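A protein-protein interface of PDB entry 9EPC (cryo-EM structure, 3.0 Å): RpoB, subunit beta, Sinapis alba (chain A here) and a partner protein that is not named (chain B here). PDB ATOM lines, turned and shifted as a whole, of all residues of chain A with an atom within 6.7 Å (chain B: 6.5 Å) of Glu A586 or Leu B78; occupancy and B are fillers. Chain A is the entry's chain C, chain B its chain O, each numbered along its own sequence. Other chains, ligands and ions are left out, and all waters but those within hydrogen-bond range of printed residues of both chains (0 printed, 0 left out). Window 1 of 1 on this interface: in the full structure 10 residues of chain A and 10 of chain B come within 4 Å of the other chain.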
ATOM      1  N   ALA A 583     -14.061  19.880  15.197  1.00  0.00           N
ATOM      2  CA  ALA A 583     -15.153  19.555  14.290  1.00  0.00           C
ATOM      3  C   ALA A 583     -15.048  20.395  13.026  1.00  0.00           C
ATOM      4  O   ALA A 583     -15.062  21.628  13.087  1.00  0.00           O
ATOM      5  CB  ALA A 583     -16.496  19.787  14.974  1.00  0.00           C
ATOM      6  N   GLU A 584     -14.936  19.727  11.884  1.00  0.00           N
ATOM      7  CA  GLU A 584     -14.952  20.388  10.588  1.00  0.00           C
ATOM      8  C   GLU A 584     -16.363  20.576  10.055  1.00  0.00           C
ATOM      9  O   GLU A 584     -16.535  21.118   8.959  1.00  0.00           O
ATOM     10  CB  GLU A 584     -14.117  19.593   9.582  1.00  0.00           C
ATOM     11  CG  GLU A 584     -14.555  18.148   9.429  1.00  0.00           C
ATOM     12  CD  GLU A 584     -13.569  17.325   8.628  1.00  0.00           C
ATOM     13  OE1 GLU A 584     -12.495  17.857   8.275  1.00  0.00           O
ATOM     14  OE2 GLU A 584     -13.866  16.145   8.350  1.00  0.00           O
ATOM     15  N   HIS A 585     -17.369  20.133  10.803  1.00  0.00           N
ATOM     16  CA  HIS A 585     -18.763  20.253  10.416  1.00  0.00           C
ATOM     17  C   HIS A 585     -19.574  20.517  11.675  1.00  0.00           C
ATOM     18  O   HIS A 585     -19.192  20.099  12.770  1.00  0.00           O
ATOM     19  CB  HIS A 585     -19.246  18.984   9.706  1.00  0.00           C
ATOM     20  CG  HIS A 585     -20.636  19.080   9.166  1.00  0.00           C
ATOM     21  ND1 HIS A 585     -20.989  19.964   8.171  1.00  0.00           N
ATOM     22  CD2 HIS A 585     -21.760  18.391   9.473  1.00  0.00           C
ATOM     23  CE1 HIS A 585     -22.272  19.821   7.892  1.00  0.00           C
ATOM     24  NE2 HIS A 585     -22.764  18.874   8.669  1.00  0.00           N
ATOM     25  N   GLU A 586     -20.687  21.221  11.516  1.00  0.00           N
ATOM     26  CA  GLU A 586     -21.530  21.543  12.656  1.00  0.00           C
ATOM     27  C   GLU A 586     -22.620  20.494  12.825  1.00  0.00           C
ATOM     28  O   GLU A 586     -22.938  19.738  11.905  1.00  0.00           O
ATOM     29  CB  GLU A 586     -22.158  22.927  12.491  1.00  0.00           C
ATOM     30  CG  GLU A 586     -23.477  22.931  11.738  1.00  0.00           C
ATOM     31  CD  GLU A 586     -23.339  22.497  10.293  1.00  0.00           C
ATOM     32  OE1 GLU A 586     -22.225  22.601   9.739  1.00  0.00           O
ATOM     33  OE2 GLU A 586     -24.347  22.053   9.709  1.00  0.00           O
ATOM     34  N   GLY A 587     -23.190  20.450  14.018  1.00  0.00           N
ATOM     35  CA  GLY A 587     -24.288  19.559  14.303  1.00  0.00           C
ATOM     36  C   GLY A 587     -24.210  19.043  15.720  1.00  0.00           C
ATOM     37  O   GLY A 587     -23.461  19.553  16.551  1.00  0.00           O
ATOM     38  N   LYS A 588     -25.002  18.012  15.991  1.00  0.00           N
ATOM     39  CA  LYS A 588     -25.072  17.407  17.311  1.00  0.00           C
ATOM     40  C   LYS A 588     -24.138  16.207  17.403  1.00  0.00           C
ATOM     41  O   LYS A 588     -23.623  15.708  16.401  1.00  0.00           O
ATOM     42  CB  LYS A 588     -26.502  16.972  17.629  1.00  0.00           C
ATOM     43  CG  LYS A 588     -27.541  18.059  17.442  1.00  0.00           C
ATOM     44  CD  LYS A 588     -28.926  17.557  17.812  1.00  0.00           C
ATOM     45  CE  LYS A 588     -29.975  18.640  17.631  1.00  0.00           C
ATOM     46  NZ  LYS A 588     -29.702  19.823  18.491  1.00  0.00           N
ATOM     47  N   LEU A 599     -20.827  12.537  14.784  1.00  0.00           N
ATOM     48  CA  LEU A 599     -21.399  13.874  14.709  1.00  0.00           C
ATOM     49  C   LEU A 599     -22.324  13.948  13.505  1.00  0.00           C
ATOM     50  O   LEU A 599     -21.942  13.546  12.401  1.00  0.00           O
ATOM     51  CB  LEU A 599     -20.298  14.934  14.610  1.00  0.00           C
ATOM     52  CG  LEU A 599     -20.710  16.405  14.556  1.00  0.00           C
ATOM     53  CD1 LEU A 599     -19.737  17.241  15.360  1.00  0.00           C
ATOM     54  CD2 LEU A 599     -20.765  16.903  13.122  1.00  0.00           C
ATOM     55  N   SER A 600     -23.532  14.462  13.717  1.00  0.00           N
ATOM     56  CA  SER A 600     -24.530  14.578  12.665  1.00  0.00           C
ATOM     57  C   SER A 600     -24.963  16.027  12.528  1.00  0.00           C
ATOM     58  O   SER A 600     -25.285  16.681  13.523  1.00  0.00           O
ATOM     59  CB  SER A 600     -25.746  13.698  12.955  1.00  0.00           C
ATOM     60  OG  SER A 600     -26.726  13.837  11.941  1.00  0.00           O
ATOM     61  N   GLY A 601     -24.981  16.517  11.292  1.00  0.00           N
ATOM     62  CA  GLY A 601     -25.429  17.863  11.001  1.00  0.00           C
ATOM     63  C   GLY A 601     -25.700  18.040   9.524  1.00  0.00           C
ATOM     64  O   GLY A 601     -24.957  17.512   8.690  1.00  0.00           O
ATOM     65  N   ASN A 602     -26.756  18.781   9.187  1.00  0.00           N
ATOM     66  CA  ASN A 602     -27.187  18.957   7.802  1.00  0.00           C
ATOM     67  C   ASN A 602     -27.410  17.601   7.136  1.00  0.00           C
ATOM     68  O   ASN A 602     -26.861  17.300   6.074  1.00  0.00           O
ATOM     69  CB  ASN A 602     -26.182  19.804   7.018  1.00  0.00           C
ATOM     70  CG  ASN A 602     -26.713  20.240   5.668  1.00  0.00           C
ATOM     71  OD1 ASN A 602     -27.922  20.276   5.447  1.00  0.00           O
ATOM     72  ND2 ASN A 602     -25.809  20.573   4.757  1.00  0.00           N
ATOM     73  N   ASN A 604     -26.154  14.955   7.444  1.00  0.00           N
ATOM     74  CA  ASN A 604     -24.913  14.256   7.146  1.00  0.00           C
ATOM     75  C   ASN A 604     -24.229  13.883   8.450  1.00  0.00           C
ATOM     76  O   ASN A 604     -24.182  14.685   9.388  1.00  0.00           O
ATOM     77  CB  ASN A 604     -23.977  15.113   6.289  1.00  0.00           C
ATOM     78  CG  ASN A 604     -24.557  15.421   4.924  1.00  0.00           C
ATOM     79  OD1 ASN A 604     -25.361  14.657   4.392  1.00  0.00           O
ATOM     80  ND2 ASN A 604     -24.148  16.544   4.346  1.00  0.00           N
ATOM     81  N   LEU A 606     -20.729  12.239  10.408  1.00  0.00           N
ATOM     82  CA  LEU A 606     -19.287  12.077  10.301  1.00  0.00           C
ATOM     83  C   LEU A 606     -18.792  11.249  11.475  1.00  0.00           C
ATOM     84  O   LEU A 606     -19.158  11.513  12.624  1.00  0.00           O
ATOM     85  CB  LEU A 606     -18.568  13.430  10.269  1.00  0.00           C
ATOM     86  CG  LEU A 606     -18.696  14.282   9.004  1.00  0.00           C
ATOM     87  CD1 LEU A 606     -20.011  15.044   8.972  1.00  0.00           C
ATOM     88  CD2 LEU A 606     -17.518  15.236   8.885  1.00  0.00           C
ATOM     89  N   ILE A 634     -22.619  21.120  18.337  1.00  0.00           N
ATOM     90  CA  ILE A 634     -21.261  21.600  18.115  1.00  0.00           C
ATOM     91  C   ILE A 634     -21.256  22.518  16.902  1.00  0.00           C
ATOM     92  O   ILE A 634     -21.809  22.170  15.853  1.00  0.00           O
ATOM     93  CB  ILE A 634     -20.276  20.435  17.917  1.00  0.00           C
ATOM     94  CG1 ILE A 634     -20.256  19.539  19.154  1.00  0.00           C
ATOM     95  CG2 ILE A 634     -18.883  20.955  17.635  1.00  0.00           C
ATOM     96  CD1 ILE A 634     -19.878  20.267  20.418  1.00  0.00           C
ATOM     97  N   LYS A 635     -20.639  23.685  17.050  1.00  0.00           N
ATOM     98  CA  LYS A 635     -20.390  24.579  15.932  1.00  0.00           C
ATOM     99  C   LYS A 635     -19.108  24.169  15.221  1.00  0.00           C
ATOM    100  O   LYS A 635     -18.198  23.599  15.828  1.00  0.00           O
ATOM    101  CB  LYS A 635     -20.279  26.027  16.409  1.00  0.00           C
ATOM    102  CG  LYS A 635     -21.558  26.582  16.998  1.00  0.00           C
ATOM    103  CD  LYS A 635     -21.314  27.884  17.735  1.00  0.00           C
ATOM    104  CE  LYS A 635     -20.667  28.918  16.840  1.00  0.00           C
ATOM    105  NZ  LYS A 635     -20.517  30.221  17.540  1.00  0.00           N
ATOM    106  N   LYS A 636     -19.045  24.454  13.923  1.00  0.00           N
ATOM    107  CA  LYS A 636     -17.851  24.128  13.158  1.00  0.00           C
ATOM    108  C   LYS A 636     -16.647  24.861  13.727  1.00  0.00           C
ATOM    109  O   LYS A 636     -16.704  26.066  13.987  1.00  0.00           O
ATOM    110  CB  LYS A 636     -18.037  24.495  11.688  1.00  0.00           C
ATOM    111  CG  LYS A 636     -16.770  24.335  10.865  1.00  0.00           C
ATOM    112  CD  LYS A 636     -16.976  24.749   9.424  1.00  0.00           C
ATOM    113  CE  LYS A 636     -15.713  24.531   8.613  1.00  0.00           C
ATOM    114  NZ  LYS A 636     -14.570  25.307   9.156  1.00  0.00           N
ATOM    115  N   GLY A 637     -15.554  24.132  13.919  1.00  0.00           N
ATOM    116  CA  GLY A 637     -14.341  24.690  14.468  1.00  0.00           C
ATOM    117  C   GLY A 637     -14.189  24.532  15.964  1.00  0.00           C
ATOM    118  O   GLY A 637     -13.103  24.806  16.488  1.00  0.00           O
ATOM    119  N   ARG B  74     -17.261  23.183   4.846  1.00  0.00           N
ATOM    120  CA  ARG B  74     -18.499  23.645   5.453  1.00  0.00           C
ATOM    121  C   ARG B  74     -18.429  25.143   5.725  1.00  0.00           C
ATOM    122  O   ARG B  74     -17.384  25.670   6.117  1.00  0.00           O
ATOM    123  CB  ARG B  74     -18.755  22.879   6.749  1.00  0.00           C
ATOM    124  CG  ARG B  74     -20.046  23.237   7.450  1.00  0.00           C
ATOM    125  CD  ARG B  74     -21.240  22.943   6.570  1.00  0.00           C
ATOM    126  NE  ARG B  74     -22.493  23.287   7.230  1.00  0.00           N
ATOM    127  CZ  ARG B  74     -23.668  23.335   6.621  1.00  0.00           C
ATOM    128  NH1 ARG B  74     -23.788  23.076   5.330  1.00  0.00           N
ATOM    129  NH2 ARG B  74     -24.751  23.654   7.324  1.00  0.00           N
ATOM    130  N   GLU B  75     -19.542  25.833   5.497  1.00  0.00           N
ATOM    131  CA  GLU B  75     -19.605  27.254   5.803  1.00  0.00           C
ATOM    132  C   GLU B  75     -19.468  27.469   7.304  1.00  0.00           C
ATOM    133  O   GLU B  75     -20.045  26.732   8.108  1.00  0.00           O
ATOM    134  CB  GLU B  75     -20.921  27.859   5.311  1.00  0.00           C
ATOM    135  CG  GLU B  75     -21.332  27.453   3.903  1.00  0.00           C
ATOM    136  CD  GLU B  75     -22.195  26.208   3.886  1.00  0.00           C
ATOM    137  OE1 GLU B  75     -22.007  25.342   4.761  1.00  0.00           O
ATOM    138  OE2 GLU B  75     -23.070  26.099   3.002  1.00  0.00           O
ATOM    139  N   ASP B  76     -18.698  28.488   7.682  1.00  0.00           N
ATOM    140  CA  ASP B  76     -18.457  28.744   9.095  1.00  0.00           C
ATOM    141  C   ASP B  76     -19.678  29.313   9.801  1.00  0.00           C
ATOM    142  O   ASP B  76     -19.810  29.141  11.016  1.00  0.00           O
ATOM    143  CB  ASP B  76     -17.279  29.700   9.260  1.00  0.00           C
ATOM    144  CG  ASP B  76     -16.078  29.288   8.440  1.00  0.00           C
ATOM    145  OD1 ASP B  76     -16.136  29.407   7.199  1.00  0.00           O
ATOM    146  OD2 ASP B  76     -15.076  28.842   9.035  1.00  0.00           O
ATOM    147  N   TYR B  77     -20.568  29.981   9.074  1.00  0.00           N
ATOM    148  CA  TYR B  77     -21.692  30.685   9.673  1.00  0.00           C
ATOM    149  C   TYR B  77     -22.988  30.227   9.027  1.00  0.00           C
ATOM    150  O   TYR B  77     -23.077  30.143   7.797  1.00  0.00           O
ATOM    151  CB  TYR B  77     -21.521  32.197   9.524  1.00  0.00           C
ATOM    152  CG  TYR B  77     -20.211  32.689  10.084  1.00  0.00           C
ATOM    153  CD1 TYR B  77     -20.095  33.030  11.422  1.00  0.00           C
ATOM    154  CD2 TYR B  77     -19.088  32.798   9.281  1.00  0.00           C
ATOM    155  CE1 TYR B  77     -18.901  33.474  11.942  1.00  0.00           C
ATOM    156  CE2 TYR B  77     -17.888  33.240   9.793  1.00  0.00           C
ATOM    157  CZ  TYR B  77     -17.801  33.576  11.125  1.00  0.00           C
ATOM    158  OH  TYR B  77     -16.608  34.018  11.643  1.00  0.00           O
ATOM    159  N   LEU B  78     -23.987  29.935   9.856  1.00  0.00           N
ATOM    160  CA  LEU B  78     -25.281  29.479   9.373  1.00  0.00           C
ATOM    161  C   LEU B  78     -26.336  30.575   9.350  1.00  0.00           C
ATOM    162  O   LEU B  78     -27.304  30.461   8.592  1.00  0.00           O
ATOM    163  CB  LEU B  78     -25.788  28.319  10.235  1.00  0.00           C
ATOM    164  CG  LEU B  78     -24.851  27.119  10.353  1.00  0.00           C
ATOM    165  CD1 LEU B  78     -25.514  26.007  11.139  1.00  0.00           C
ATOM    166  CD2 LEU B  78     -24.433  26.635   8.978  1.00  0.00           C
ATOM    167  N   VAL B  79     -26.178  31.621  10.154  1.00  0.00           N
ATOM    168  CA  VAL B  79     -27.149  32.710  10.200  1.00  0.00           C
ATOM    169  C   VAL B  79     -26.928  33.588   8.975  1.00  0.00           C
ATOM    170  O   VAL B  79     -25.896  34.253   8.852  1.00  0.00           O
ATOM    171  CB  VAL B  79     -27.026  33.518  11.495  1.00  0.00           C
ATOM    172  CG1 VAL B  79     -28.030  34.651  11.502  1.00  0.00           C
ATOM    173  CG2 VAL B  79     -27.235  32.616  12.696  1.00  0.00           C
ATOM    174  N   ARG B  80     -27.899  33.597   8.069  1.00  0.00           N
ATOM    175  CA  ARG B  80     -27.780  34.304   6.803  1.00  0.00           C
ATOM    176  C   ARG B  80     -28.242  35.747   6.957  1.00  0.00           C
ATOM    177  O   ARG B  80     -29.297  36.009   7.543  1.00  0.00           O
ATOM    178  CB  ARG B  80     -28.602  33.599   5.725  1.00  0.00           C
ATOM    179  CG  ARG B  80     -28.643  34.323   4.393  1.00  0.00           C
ATOM    180  CD  ARG B  80     -29.498  33.577   3.378  1.00  0.00           C
ATOM    181  NE  ARG B  80     -30.903  33.521   3.765  1.00  0.00           N
ATOM    182  CZ  ARG B  80     -31.477  32.486   4.362  1.00  0.00           C
ATOM    183  NH1 ARG B  80     -30.794  31.393   4.660  1.00  0.00           N
ATOM    184  NH2 ARG B  80     -32.770  32.547   4.666  1.00  0.00           N
ATOM    185  N   LEU B 118     -26.760  33.025  18.251  1.00  0.00           N
ATOM    186  CA  LEU B 118     -27.588  32.655  17.107  1.00  0.00           C
ATOM    187  C   LEU B 118     -26.943  31.537  16.302  1.00  0.00           C
ATOM    188  O   LEU B 118     -27.631  30.616  15.847  1.00  0.00           O
ATOM    189  CB  LEU B 118     -27.853  33.869  16.221  1.00  0.00           C
ATOM    190  CG  LEU B 118     -28.953  34.819  16.692  1.00  0.00           C
ATOM    191  CD1 LEU B 118     -30.116  34.051  17.290  1.00  0.00           C
ATOM    192  CD2 LEU B 118     -28.414  35.802  17.685  1.00  0.00           C
ATOM    193  N   GLU B 119     -25.624  31.597  16.115  1.00  0.00           N
ATOM    194  CA  GLU B 119     -24.929  30.500  15.455  1.00  0.00           C
ATOM    195  C   GLU B 119     -25.106  29.206  16.234  1.00  0.00           C
ATOM    196  O   GLU B 119     -25.376  28.151  15.650  1.00  0.00           O
ATOM    197  CB  GLU B 119     -23.445  30.830  15.305  1.00  0.00           C
ATOM    198  CG  GLU B 119     -23.158  32.177  14.671  1.00  0.00           C
ATOM    199  CD  GLU B 119     -23.237  32.144  13.161  1.00  0.00           C
ATOM    200  OE1 GLU B 119     -23.259  31.035  12.591  1.00  0.00           O
ATOM    201  OE2 GLU B 119     -23.274  33.229  12.545  1.00  0.00           O
ATOM    202  N   ALA B 122     -28.706  28.241  15.776  1.00  0.00           N
ATOM    203  CA  ALA B 122     -28.954  27.709  14.443  1.00  0.00           C
ATOM    204  C   ALA B 122     -28.528  26.253  14.331  1.00  0.00           C
ATOM    205  O   ALA B 122     -29.121  25.491  13.561  1.00  0.00           O
ATOM    206  CB  ALA B 122     -28.232  28.554  13.395  1.00  0.00           C
ATOM    207  N   VAL B 123     -27.501  25.849  15.079  1.00  0.00           N
ATOM    208  CA  VAL B 123     -27.111  24.444  15.097  1.00  0.00           C
ATOM    209  C   VAL B 123     -28.180  23.605  15.784  1.00  0.00           C
ATOM    210  O   VAL B 123     -28.493  22.493  15.343  1.00  0.00           O
ATOM    211  CB  VAL B 123     -25.738  24.277  15.770  1.00  0.00           C
ATOM    212  CG1 VAL B 123     -25.348  22.811  15.814  1.00  0.00           C
ATOM    213  CG2 VAL B 123     -24.690  25.081  15.030  1.00  0.00           C
ATOM    214  N   GLU B 126     -31.632  23.064  13.115  1.00  0.00           N
ATOM    215  CA  GLU B 126     -31.039  22.961  11.785  1.00  0.00           C
ATOM    216  C   GLU B 126     -32.031  23.381  10.708  1.00  0.00           C
ATOM    217  O   GLU B 126     -31.729  24.232   9.864  1.00  0.00           O
ATOM    218  CB  GLU B 126     -30.552  21.534  11.536  1.00  0.00           C
ATOM    219  CG  GLU B 126     -29.563  21.015  12.565  1.00  0.00           C
ATOM    220  CD  GLU B 126     -30.238  20.408  13.779  1.00  0.00           C
ATOM    221  OE1 GLU B 126     -29.572  19.646  14.512  1.00  0.00           O
ATOM    222  OE2 GLU B 126     -31.435  20.688  14.000  1.00  0.00           O
ATOM    223  N   ILE B 131     -33.150  31.093  11.066  1.00  0.00           N
ATOM    224  CA  ILE B 131     -32.573  32.247  11.742  1.00  0.00           C
ATOM    225  C   ILE B 131     -31.887  33.112  10.698  1.00  0.00           C
ATOM    226  O   ILE B 131     -31.021  32.633   9.956  1.00  0.00           O
ATOM    227  CB  ILE B 131     -31.588  31.827  12.842  1.00  0.00           C
ATOM    228  CG1 ILE B 131     -32.290  30.953  13.879  1.00  0.00           C
ATOM    229  CG2 ILE B 131     -30.983  33.048  13.505  1.00  0.00           C
ATOM    230  CD1 ILE B 131     -31.405  30.559  15.031  1.00  0.00           C
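The guanidinium group (NE) of Arg B74 is in salt-bridge range of the side-chain carboxylate (OE1) of Glu A586. The side-chain amide nitrogen (ND2) of Asn A602 lies close to the guanidinium group (NH1) of Arg B74 (3.3 Å). The side-chain carboxylate of Asp B76 lies within salt-bridge range of the side-chain amino group of Lys A636, 3.6 Å away. The side-chain amino group of Lys A588 is in salt-bridge range of the side-chain carboxylate of Glu B126 (3.99 Å).
The guanidinium group of Arg B74 lies within salt-bridge range of the side-chain carboxylate of Glu B75, 2.9 Å away. ND1 of His A585 is in hydrogen-bond range of OE1 of Glu A586, 3.3 Å away. O of Gly A601 sits at hydrogen-bond distance from NE2 of His A585. The backbone carbonyl oxygen of Gly A587 is in hydrogen-bond range of the backbone NH of Ile A634 (2.5 Å). O of Ser A600 lies within hydrogen-bond range of N of Lys A588, at 2.8 Å. O of Asn A602 lies close to ND2 of Asn A604, at 3.3 Å.
Among the printed residues, merely in contact across the chains: Glu A584 with Arg B74 (3.6 Å), His A585 with Arg B74 (3.4 Å), Glu A586 with Leu B78 (3.7 Å), Gly A587 with Val B123 (3.7 Å), Ile A634 with Val B123 (3.6 Å), Lys A635 with Glu B119 (3.7 Å), Lys A635 with Val B123 (3.99 Å), Lys A636 with Arg B74 (3.2 Å) and Lys A636 with Glu B75 (3.9 Å).
Printed residues of chain B within 4 Å of Glu A584: Arg B74. Of chain B, only Arg B74 (2.6 Å) and Leu B78 (3.7 Å) come within 4 Å of Glu A586. Printed residues of chain B within 4 Å of Lys A636: Arg B74 (3.2 Å), Glu B75 (3.9 Å) and Asp B76 (3.6 Å). Gly A637 touches none of the printed residues of chain B. Of the printed residues of chain A, Glu B75 touches Lys A636. Leu B78 touches just one residue of chain A: Glu A586.
Printed residues of chain A that touch a printed residue of chain B: Glu A584, His A585, Glu A586, Gly A587, Lys A588, Asn A602, Ile A634, Lys A635 and Lys A636. Hydrophobic or aromatic side chains of chain A within 4 Å of the printed part of chain B: His A585. Among the printed residues, 13 pairs touch across the chains.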
